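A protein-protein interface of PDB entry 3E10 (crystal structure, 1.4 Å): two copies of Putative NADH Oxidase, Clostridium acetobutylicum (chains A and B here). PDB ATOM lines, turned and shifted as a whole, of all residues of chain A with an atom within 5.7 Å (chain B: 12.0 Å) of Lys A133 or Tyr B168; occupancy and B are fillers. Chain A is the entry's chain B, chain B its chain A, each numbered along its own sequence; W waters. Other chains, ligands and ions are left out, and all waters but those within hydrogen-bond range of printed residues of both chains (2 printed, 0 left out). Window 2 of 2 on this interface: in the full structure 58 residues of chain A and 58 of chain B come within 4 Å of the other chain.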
ATOM      1  N   GLU A  44       1.510  -7.193 -13.921  1.00  0.00           N
ATOM      2  CA  GLU A  44       0.139  -7.295 -14.458  1.00  0.00           C
ATOM      3  C   GLU A  44      -0.628  -6.120 -13.889  1.00  0.00           C
ATOM      4  O   GLU A  44      -0.327  -5.688 -12.799  1.00  0.00           O
ATOM      5  CB  GLU A  44      -0.515  -8.602 -13.952  1.00  0.00           C
ATOM      6  CG  GLU A  44       0.150  -9.889 -14.452  1.00  0.00           C
ATOM      7  CD  GLU A  44      -0.139 -10.225 -15.898  1.00  0.00           C
ATOM      8  OE1 GLU A  44      -0.974  -9.524 -16.552  1.00  0.00           O
ATOM      9  OE2 GLU A  44       0.485 -11.206 -16.416  1.00  0.00           O
ATOM     10  N   ILE A  46      -4.608  -4.253 -13.380  1.00  0.00           N
ATOM     11  CA  ILE A  46      -6.069  -4.202 -13.506  1.00  0.00           C
ATOM     12  C   ILE A  46      -6.450  -2.712 -13.596  1.00  0.00           C
ATOM     13  O   ILE A  46      -6.103  -1.910 -12.735  1.00  0.00           O
ATOM     14  CB  ILE A  46      -6.811  -4.839 -12.330  1.00  0.00           C
ATOM     15  CG1 ILE A  46      -6.335  -6.257 -12.056  1.00  0.00           C
ATOM     16  CG2 ILE A  46      -8.347  -4.840 -12.604  1.00  0.00           C
ATOM     17  CD1 ILE A  46      -6.897  -6.879 -10.746  1.00  0.00           C
ATOM     18  N   LEU A  77       0.148  -5.533  -9.925  1.00  0.00           N
ATOM     19  CA  LEU A  77       0.302  -6.874  -9.430  1.00  0.00           C
ATOM     20  C   LEU A  77       1.561  -7.477 -10.020  1.00  0.00           C
ATOM     21  O   LEU A  77       1.981  -7.056 -11.085  1.00  0.00           O
ATOM     22  CB  LEU A  77      -0.901  -7.727  -9.873  1.00  0.00           C
ATOM     23  CG  LEU A  77      -2.344  -7.180  -9.759  1.00  0.00           C
ATOM     24  CD1 LEU A  77      -3.266  -8.010 -10.699  1.00  0.00           C
ATOM     25  CD2 LEU A  77      -2.805  -7.370  -8.389  1.00  0.00           C
ATOM     26  N   ASP A  79       3.359 -11.385 -10.977  1.00  0.00           N
ATOM     27  CA  ASP A  79       3.114 -12.818 -11.143  1.00  0.00           C
ATOM     28  C   ASP A  79       4.364 -13.610 -10.751  1.00  0.00           C
ATOM     29  O   ASP A  79       5.428 -13.451 -11.357  1.00  0.00           O
ATOM     30  CB  ASP A  79       2.790 -13.087 -12.600  1.00  0.00           C
ATOM     31  CG  ASP A  79       2.433 -14.532 -12.877  1.00  0.00           C
ATOM     32  OD1 ASP A  79       2.488 -15.372 -11.952  1.00  0.00           O
ATOM     33  OD2 ASP A  79       2.110 -14.827 -14.047  1.00  0.00           O
ATOM     34  N   LYS A  82       6.362 -15.371 -13.371  1.00  0.00           N
ATOM     35  CA  LYS A  82       7.248 -14.610 -14.229  1.00  0.00           C
ATOM     36  C   LYS A  82       8.574 -14.255 -13.562  1.00  0.00           C
ATOM     37  O   LYS A  82       9.456 -13.690 -14.205  1.00  0.00           O
ATOM     38  CB  LYS A  82       6.549 -13.341 -14.704  1.00  0.00           C
ATOM     39  CG  LYS A  82       5.329 -13.637 -15.532  1.00  0.00           C
ATOM     40  CD  LYS A  82       4.688 -12.364 -16.035  1.00  0.00           C
ATOM     41  CE  LYS A  82       3.594 -12.668 -17.060  1.00  0.00           C
ATOM     42  NZ  LYS A  82       2.345 -13.160 -16.416  1.00  0.00           N
ATOM     43  N   PHE A 130     -10.466  -9.124  -5.904  1.00  0.00           N
ATOM     44  CA  PHE A 130     -10.297  -9.572  -7.265  1.00  0.00           C
ATOM     45  C   PHE A 130     -10.192 -11.103  -7.425  1.00  0.00           C
ATOM     46  O   PHE A 130      -9.967 -11.586  -8.531  1.00  0.00           O
ATOM     47  CB  PHE A 130      -9.047  -8.882  -7.843  1.00  0.00           C
ATOM     48  CG  PHE A 130      -9.207  -7.385  -7.965  1.00  0.00           C
ATOM     49  CD1 PHE A 130     -10.007  -6.850  -8.960  1.00  0.00           C
ATOM     50  CD2 PHE A 130      -8.589  -6.530  -7.051  1.00  0.00           C
ATOM     51  CE1 PHE A 130     -10.189  -5.489  -9.050  1.00  0.00           C
ATOM     52  CE2 PHE A 130      -8.760  -5.153  -7.147  1.00  0.00           C
ATOM     53  CZ  PHE A 130      -9.538  -4.636  -8.145  1.00  0.00           C
ATOM     54  N   ASN A 131     -10.431 -11.837  -6.334  1.00  0.00           N
ATOM     55  CA  ASN A 131     -10.285 -13.288  -6.274  1.00  0.00           C
ATOM     56  C   ASN A 131      -9.037 -13.776  -6.989  1.00  0.00           C
ATOM     57  O   ASN A 131      -9.100 -14.580  -7.895  1.00  0.00           O
ATOM     58  CB  ASN A 131     -11.523 -13.999  -6.799  1.00  0.00           C
ATOM     59  CG  ASN A 131     -11.490 -15.466  -6.493  1.00  0.00           C
ATOM     60  OD1 ASN A 131     -11.042 -15.855  -5.412  1.00  0.00           O
ATOM     61  ND2 ASN A 131     -11.883 -16.301  -7.477  1.00  0.00           N
ATOM     62  N   LEU A 132      -7.895 -13.243  -6.585  1.00  0.00           N
ATOM     63  CA  LEU A 132      -6.676 -13.523  -7.312  1.00  0.00           C
ATOM     64  C   LEU A 132      -6.167 -14.935  -7.071  1.00  0.00           C
ATOM     65  O   LEU A 132      -6.237 -15.447  -5.963  1.00  0.00           O
ATOM     66  CB  LEU A 132      -5.564 -12.531  -6.897  1.00  0.00           C
ATOM     67  CG  LEU A 132      -5.877 -11.062  -7.169  1.00  0.00           C
ATOM     68  CD1 LEU A 132      -4.753 -10.189  -6.632  1.00  0.00           C
ATOM     69  CD2 LEU A 132      -6.123 -10.846  -8.675  1.00  0.00           C
ATOM     70  N   LYS A 133      -5.624 -15.535  -8.116  1.00  0.00           N
ATOM     71  CA  LYS A 133      -4.811 -16.748  -8.019  1.00  0.00           C
ATOM     72  C   LYS A 133      -3.644 -16.548  -7.058  1.00  0.00           C
ATOM     73  O   LYS A 133      -3.102 -15.447  -6.954  1.00  0.00           O
ATOM     74  CB  LYS A 133      -4.211 -17.082  -9.375  1.00  0.00           C
ATOM     75  CG  LYS A 133      -5.127 -17.739 -10.372  1.00  0.00           C
ATOM     76  CD  LYS A 133      -4.435 -17.936 -11.726  1.00  0.00           C
ATOM     77  CE  LYS A 133      -4.348 -16.646 -12.553  1.00  0.00           C
ATOM     78  NZ  LYS A 133      -5.603 -15.989 -12.868  1.00  0.00           N
ATOM     79  N   SER A 134      -3.212 -17.613  -6.401  1.00  0.00           N
ATOM     80  CA  SER A 134      -2.149 -17.555  -5.411  1.00  0.00           C
ATOM     81  C   SER A 134      -0.869 -16.872  -5.941  1.00  0.00           C
ATOM     82  O   SER A 134      -0.173 -16.150  -5.216  1.00  0.00           O
ATOM     83  CB  SER A 134      -1.818 -18.982  -4.981  1.00  0.00           C
ATOM     84  OG  SER A 134      -0.641 -19.025  -4.232  1.00  0.00           O
ATOM     85  N   ASN A 135      -0.584 -17.099  -7.220  1.00  0.00           N
ATOM     86  CA  ASN A 135       0.654 -16.590  -7.815  1.00  0.00           C
ATOM     87  C   ASN A 135       0.598 -15.122  -8.179  1.00  0.00           C
ATOM     88  O   ASN A 135       1.629 -14.555  -8.540  1.00  0.00           O
ATOM     89  CB  ASN A 135       1.050 -17.414  -9.040  1.00  0.00           C
ATOM     90  CG  ASN A 135      -0.057 -17.547 -10.074  1.00  0.00           C
ATOM     91  OD1 ASN A 135      -1.110 -18.131  -9.785  1.00  0.00           O
ATOM     92  ND2 ASN A 135       0.149 -16.983 -11.273  1.00  0.00           N
ATOM     93  N   ILE A 136      -0.594 -14.508  -8.113  1.00  0.00           N
ATOM     94  CA  ILE A 136      -0.738 -13.112  -8.517  1.00  0.00           C
ATOM     95  C   ILE A 136      -0.758 -12.258  -7.257  1.00  0.00           C
ATOM     96  O   ILE A 136      -1.687 -12.332  -6.448  1.00  0.00           O
ATOM     97  CB  ILE A 136      -1.974 -12.911  -9.366  1.00  0.00           C
ATOM     98  CG1 ILE A 136      -1.941 -13.818 -10.636  1.00  0.00           C
ATOM     99  CG2 ILE A 136      -2.118 -11.460  -9.771  1.00  0.00           C
ATOM    100  CD1 ILE A 136      -0.744 -13.667 -11.542  1.00  0.00           C
ATOM    101  N   LYS A 137       0.322 -11.511  -7.058  1.00  0.00           N
ATOM    102  CA  LYS A 137       0.566 -10.798  -5.821  1.00  0.00           C
ATOM    103  C   LYS A 137       0.254  -9.328  -5.953  1.00  0.00           C
ATOM    104  O   LYS A 137       0.848  -8.640  -6.803  1.00  0.00           O
ATOM    105  CB  LYS A 137       2.045 -10.919  -5.463  1.00  0.00           C
ATOM    106  CG  LYS A 137       2.448 -12.398  -5.320  1.00  0.00           C
ATOM    107  CD  LYS A 137       3.893 -12.559  -4.841  1.00  0.00           C
ATOM    108  CE  LYS A 137       4.115 -12.092  -3.402  1.00  0.00           C
ATOM    109  NZ  LYS A 137       3.452 -12.982  -2.387  1.00  0.00           N
ATOM    110  N   ASP B 159       3.054  -4.861 -23.673  1.00  0.00           N
ATOM    111  CA  ASP B 159       2.371  -6.123 -23.882  1.00  0.00           C
ATOM    112  C   ASP B 159       0.934  -5.950 -23.393  1.00  0.00           C
ATOM    113  O   ASP B 159       0.686  -5.883 -22.194  1.00  0.00           O
ATOM    114  CB  ASP B 159       3.088  -7.215 -23.115  1.00  0.00           C
ATOM    115  CG  ASP B 159       2.469  -8.603 -23.316  1.00  0.00           C
ATOM    116  OD1 ASP B 159       1.423  -8.731 -23.983  1.00  0.00           O
ATOM    117  OD2 ASP B 159       3.081  -9.572 -22.781  1.00  0.00           O
ATOM    118  N   ALA B 160      -0.006  -5.856 -24.324  1.00  0.00           N
ATOM    119  CA  ALA B 160      -1.420  -5.682 -23.993  1.00  0.00           C
ATOM    120  C   ALA B 160      -1.966  -6.846 -23.168  1.00  0.00           C
ATOM    121  O   ALA B 160      -2.959  -6.687 -22.479  1.00  0.00           O
ATOM    122  CB  ALA B 160      -2.229  -5.541 -25.250  1.00  0.00           C
ATOM    123  N   LYS B 161      -1.311  -8.009 -23.191  1.00  0.00           N
ATOM    124  CA  LYS B 161      -1.768  -9.161 -22.380  1.00  0.00           C
ATOM    125  C   LYS B 161      -1.648  -8.890 -20.884  1.00  0.00           C
ATOM    126  O   LYS B 161      -2.239  -9.605 -20.070  1.00  0.00           O
ATOM    127  CB  LYS B 161      -0.994 -10.443 -22.720  1.00  0.00           C
ATOM    128  CG  LYS B 161      -1.183 -10.942 -24.137  1.00  0.00           C
ATOM    129  CD  LYS B 161      -0.486 -12.292 -24.339  1.00  0.00           C
ATOM    130  CE  LYS B 161      -0.701 -12.818 -25.758  1.00  0.00           C
ATOM    131  NZ  LYS B 161      -2.157 -12.947 -26.126  1.00  0.00           N
ATOM    132  N   ARG B 162      -0.858  -7.884 -20.508  1.00  0.00           N
ATOM    133  CA  ARG B 162      -0.693  -7.525 -19.109  1.00  0.00           C
ATOM    134  C   ARG B 162      -1.814  -6.632 -18.606  1.00  0.00           C
ATOM    135  O   ARG B 162      -1.821  -6.252 -17.432  1.00  0.00           O
ATOM    136  CB  ARG B 162       0.647  -6.835 -18.856  1.00  0.00           C
ATOM    137  CG  ARG B 162       1.854  -7.630 -19.329  1.00  0.00           C
ATOM    138  CD  ARG B 162       1.909  -9.042 -18.826  1.00  0.00           C
ATOM    139  NE  ARG B 162       3.133  -9.710 -19.281  1.00  0.00           N
ATOM    140  CZ  ARG B 162       4.320  -9.628 -18.673  1.00  0.00           C
ATOM    141  NH1 ARG B 162       4.484  -8.971 -17.535  1.00  0.00           N
ATOM    142  NH2 ARG B 162       5.361 -10.240 -19.198  1.00  0.00           N
ATOM    143  N   ILE B 163      -2.746  -6.254 -19.485  1.00  0.00           N
ATOM    144  CA  ILE B 163      -3.835  -5.318 -19.124  1.00  0.00           C
ATOM    145  C   ILE B 163      -5.139  -6.086 -18.922  1.00  0.00           C
ATOM    146  O   ILE B 163      -5.587  -6.773 -19.816  1.00  0.00           O
ATOM    147  CB  ILE B 163      -4.022  -4.232 -20.201  1.00  0.00           C
ATOM    148  CG1 ILE B 163      -2.718  -3.470 -20.425  1.00  0.00           C
ATOM    149  CG2 ILE B 163      -5.146  -3.241 -19.812  1.00  0.00           C
ATOM    150  CD1 ILE B 163      -2.771  -2.525 -21.607  1.00  0.00           C
ATOM    151  N   HIS B 164      -5.719  -5.939 -17.730  1.00  0.00           N
ATOM    152  CA  HIS B 164      -6.941  -6.601 -17.342  1.00  0.00           C
ATOM    153  C   HIS B 164      -7.976  -5.512 -17.085  1.00  0.00           C
ATOM    154  O   HIS B 164      -7.742  -4.591 -16.284  1.00  0.00           O
ATOM    155  CB  HIS B 164      -6.692  -7.402 -16.076  1.00  0.00           C
ATOM    156  CG  HIS B 164      -5.581  -8.398 -16.197  1.00  0.00           C
ATOM    157  ND1 HIS B 164      -5.797  -9.755 -16.336  1.00  0.00           N
ATOM    158  CD2 HIS B 164      -4.243  -8.226 -16.239  1.00  0.00           C
ATOM    159  CE1 HIS B 164      -4.632 -10.370 -16.439  1.00  0.00           C
ATOM    160  NE2 HIS B 164      -3.672  -9.459 -16.393  1.00  0.00           N
ATOM    161  N   ILE B 165      -9.102  -5.588 -17.798  1.00  0.00           N
ATOM    162  CA  ILE B 165     -10.136  -4.558 -17.731  1.00  0.00           C
ATOM    163  C   ILE B 165     -11.187  -4.893 -16.660  1.00  0.00           C
ATOM    164  O   ILE B 165     -11.956  -5.884 -16.793  1.00  0.00           O
ATOM    165  CB  ILE B 165     -10.819  -4.390 -19.110  1.00  0.00           C
ATOM    166  CG1 ILE B 165      -9.809  -3.959 -20.173  1.00  0.00           C
ATOM    167  CG2 ILE B 165     -11.991  -3.424 -19.029  1.00  0.00           C
ATOM    168  CD1 ILE B 165      -9.166  -2.591 -19.936  1.00  0.00           C
ATOM    169  N   GLU B 166     -11.172  -4.079 -15.596  1.00  0.00           N
ATOM    170  CA  GLU B 166     -12.119  -4.095 -14.472  1.00  0.00           C
ATOM    171  C   GLU B 166     -11.962  -5.265 -13.504  1.00  0.00           C
ATOM    172  O   GLU B 166     -12.173  -5.116 -12.295  1.00  0.00           O
ATOM    173  CB  GLU B 166     -13.583  -3.993 -14.951  1.00  0.00           C
ATOM    174  CG  GLU B 166     -13.902  -2.748 -15.792  1.00  0.00           C
ATOM    175  CD  GLU B 166     -13.749  -1.402 -15.067  1.00  0.00           C
ATOM    176  OE1 GLU B 166     -13.817  -1.355 -13.835  1.00  0.00           O
ATOM    177  OE2 GLU B 166     -13.593  -0.375 -15.769  1.00  0.00           O
ATOM    178  N   LYS B 167     -11.596  -6.416 -14.038  1.00  0.00           N
ATOM    179  CA  LYS B 167     -11.422  -7.640 -13.276  1.00  0.00           C
ATOM    180  C   LYS B 167     -10.189  -8.316 -13.845  1.00  0.00           C
ATOM    181  O   LYS B 167      -9.765  -8.018 -14.959  1.00  0.00           O
ATOM    182  CB  LYS B 167     -12.652  -8.560 -13.401  1.00  0.00           C
ATOM    183  CG  LYS B 167     -12.950  -9.019 -14.805  1.00  0.00           C
ATOM    184  CD  LYS B 167     -14.245  -9.841 -14.898  1.00  0.00           C
ATOM    185  CE  LYS B 167     -14.530 -10.175 -16.347  1.00  0.00           C
ATOM    186  NZ  LYS B 167     -15.543 -11.245 -16.465  1.00  0.00           N
ATOM    187  N   TYR B 168      -9.579  -9.193 -13.068  1.00  0.00           N
ATOM    188  CA  TYR B 168      -8.446  -9.939 -13.571  1.00  0.00           C
ATOM    189  C   TYR B 168      -8.862 -10.885 -14.713  1.00  0.00           C
ATOM    190  O   TYR B 168      -8.129 -11.090 -15.684  1.00  0.00           O
ATOM    191  CB  TYR B 168      -7.793 -10.767 -12.456  1.00  0.00           C
ATOM    192  CG  TYR B 168      -6.379 -11.149 -12.833  1.00  0.00           C
ATOM    193  CD1 TYR B 168      -5.342 -10.236 -12.667  1.00  0.00           C
ATOM    194  CD2 TYR B 168      -6.096 -12.373 -13.412  1.00  0.00           C
ATOM    195  CE1 TYR B 168      -4.053 -10.551 -13.034  1.00  0.00           C
ATOM    196  CE2 TYR B 168      -4.812 -12.692 -13.795  1.00  0.00           C
ATOM    197  CZ  TYR B 168      -3.786 -11.765 -13.598  1.00  0.00           C
ATOM    198  OH  TYR B 168      -2.502 -12.066 -14.010  1.00  0.00           O
ATOM    199  OXT TYR B 168      -9.921 -11.533 -14.675  1.00  0.00           O
HETATM  200  O   HOH W   1     -10.912 -10.057 -10.640  1.00  0.00           O
HETATM  201  O   HOH W   2      -0.917 -11.745 -18.660  1.00  0.00           O
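A ring nitrogen (NE2) of His B164 is in hydrogen-bond range of the side-chain carboxylate (OE1) of Glu A44.
O of Arg B162 sits close to OE1 of Glu A44 (3.5 Å).
The backbone NH (N) of Lys B161 lies within hydrogen-bond range of the side-chain carboxylate (OD1) of Asp B159.
The side-chain carboxylate (OD2) of Asp B159 lies within salt-bridge range of the guanidinium group (NE) of Arg B162, 3.5 Å away.
ND1 of His B164 sits at hydrogen-bond distance from O of Tyr B168, at 2.8 Å.
The backbone carbonyl oxygen (O) of Leu A77 lies within hydrogen-bond range of the backbone NH (N) of Glu A44 (2.9 Å).
NZ of Lys A82 is in salt-bridge range of OE2 of Glu A44, 2.7 Å away.
The side-chain carboxylate (OD2) of Asp A79 is in salt-bridge range of the side-chain amino group (NZ) of Lys A82 (2.9 Å).
Among the printed residues, pairs that only touch across the chains: Glu A44 with Lys B161 (3.7 Å), Glu A44 with Tyr B168 (3.5 Å), Ile A46 with His B164 (3.3 Å), Ile A46 with Glu B166 (3.7 Å), Ile A46 with Lys B167 (3.9 Å), Leu A77 with Tyr B168 (3.5 Å), Lys A82 with Arg B162 (3.5 Å), Phe A130 with Glu B166 (3.8 Å), Lys A133 with Tyr B168 (3.5 Å) and Ile A136 with Tyr B168 (3.4 Å).
Of the printed residues of chain B, Lys A133 touches Tyr B168 (3.5 Å).
Printed residues of chain A within 4 Å of Tyr B168: Glu A44 (3.5 Å), Leu A77 (3.5 Å), Lys A133 (3.5 Å) and Ile A136 (3.4 Å).
Leu A77 touches one residue of chain B.
Printed residues of chain B within 4 Å of Phe A130: Glu B166 (3.8 Å).
No residue of chain B comes within 4 Å of Asn A135.
Ile A136 touches just one residue of chain B: Tyr B168 (3.4 Å).
Of the printed residues of chain A, Glu B166 touches Ile A46 and Phe A130.
Printed residues of chain B within 4 Å of Glu A44: Lys B161, Arg B162, His B164 and Tyr B168.
Of the printed residues of chain A, Lys B167 touches Ile A46.
Printed residues of chain A within 4 Å of His B164: Glu A44 and Ile A46.
Of the printed residues of chain A, Arg B162 touches Glu A44 (3.3 Å) and Lys A82 (3.5 Å).
Asp A79 touches none of the printed residues of chain B.
The nearest printed residue of chain B that does not touch Lys A133 is His B164 (6.7 Å).
Of the 10 printed residues of chain B, 6 touch a printed residue of chain A.
Among the printed residues, no Asp or Glu carboxylate lies within 4 Å of a Lys or Arg side-chain nitrogen of the other chain.
No position is printed for both chains.
Of the 12 pairs that touch across the chains among the printed residues, none has its exchanged pair printed and touching as well.
Water W2 bridges OE2 of Glu A44 (2.7 Å) and O of Lys B161 (2.9 Å).
Water W1 lies within hydrogen-bond range of O of Phe A130 and N of Tyr B168.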
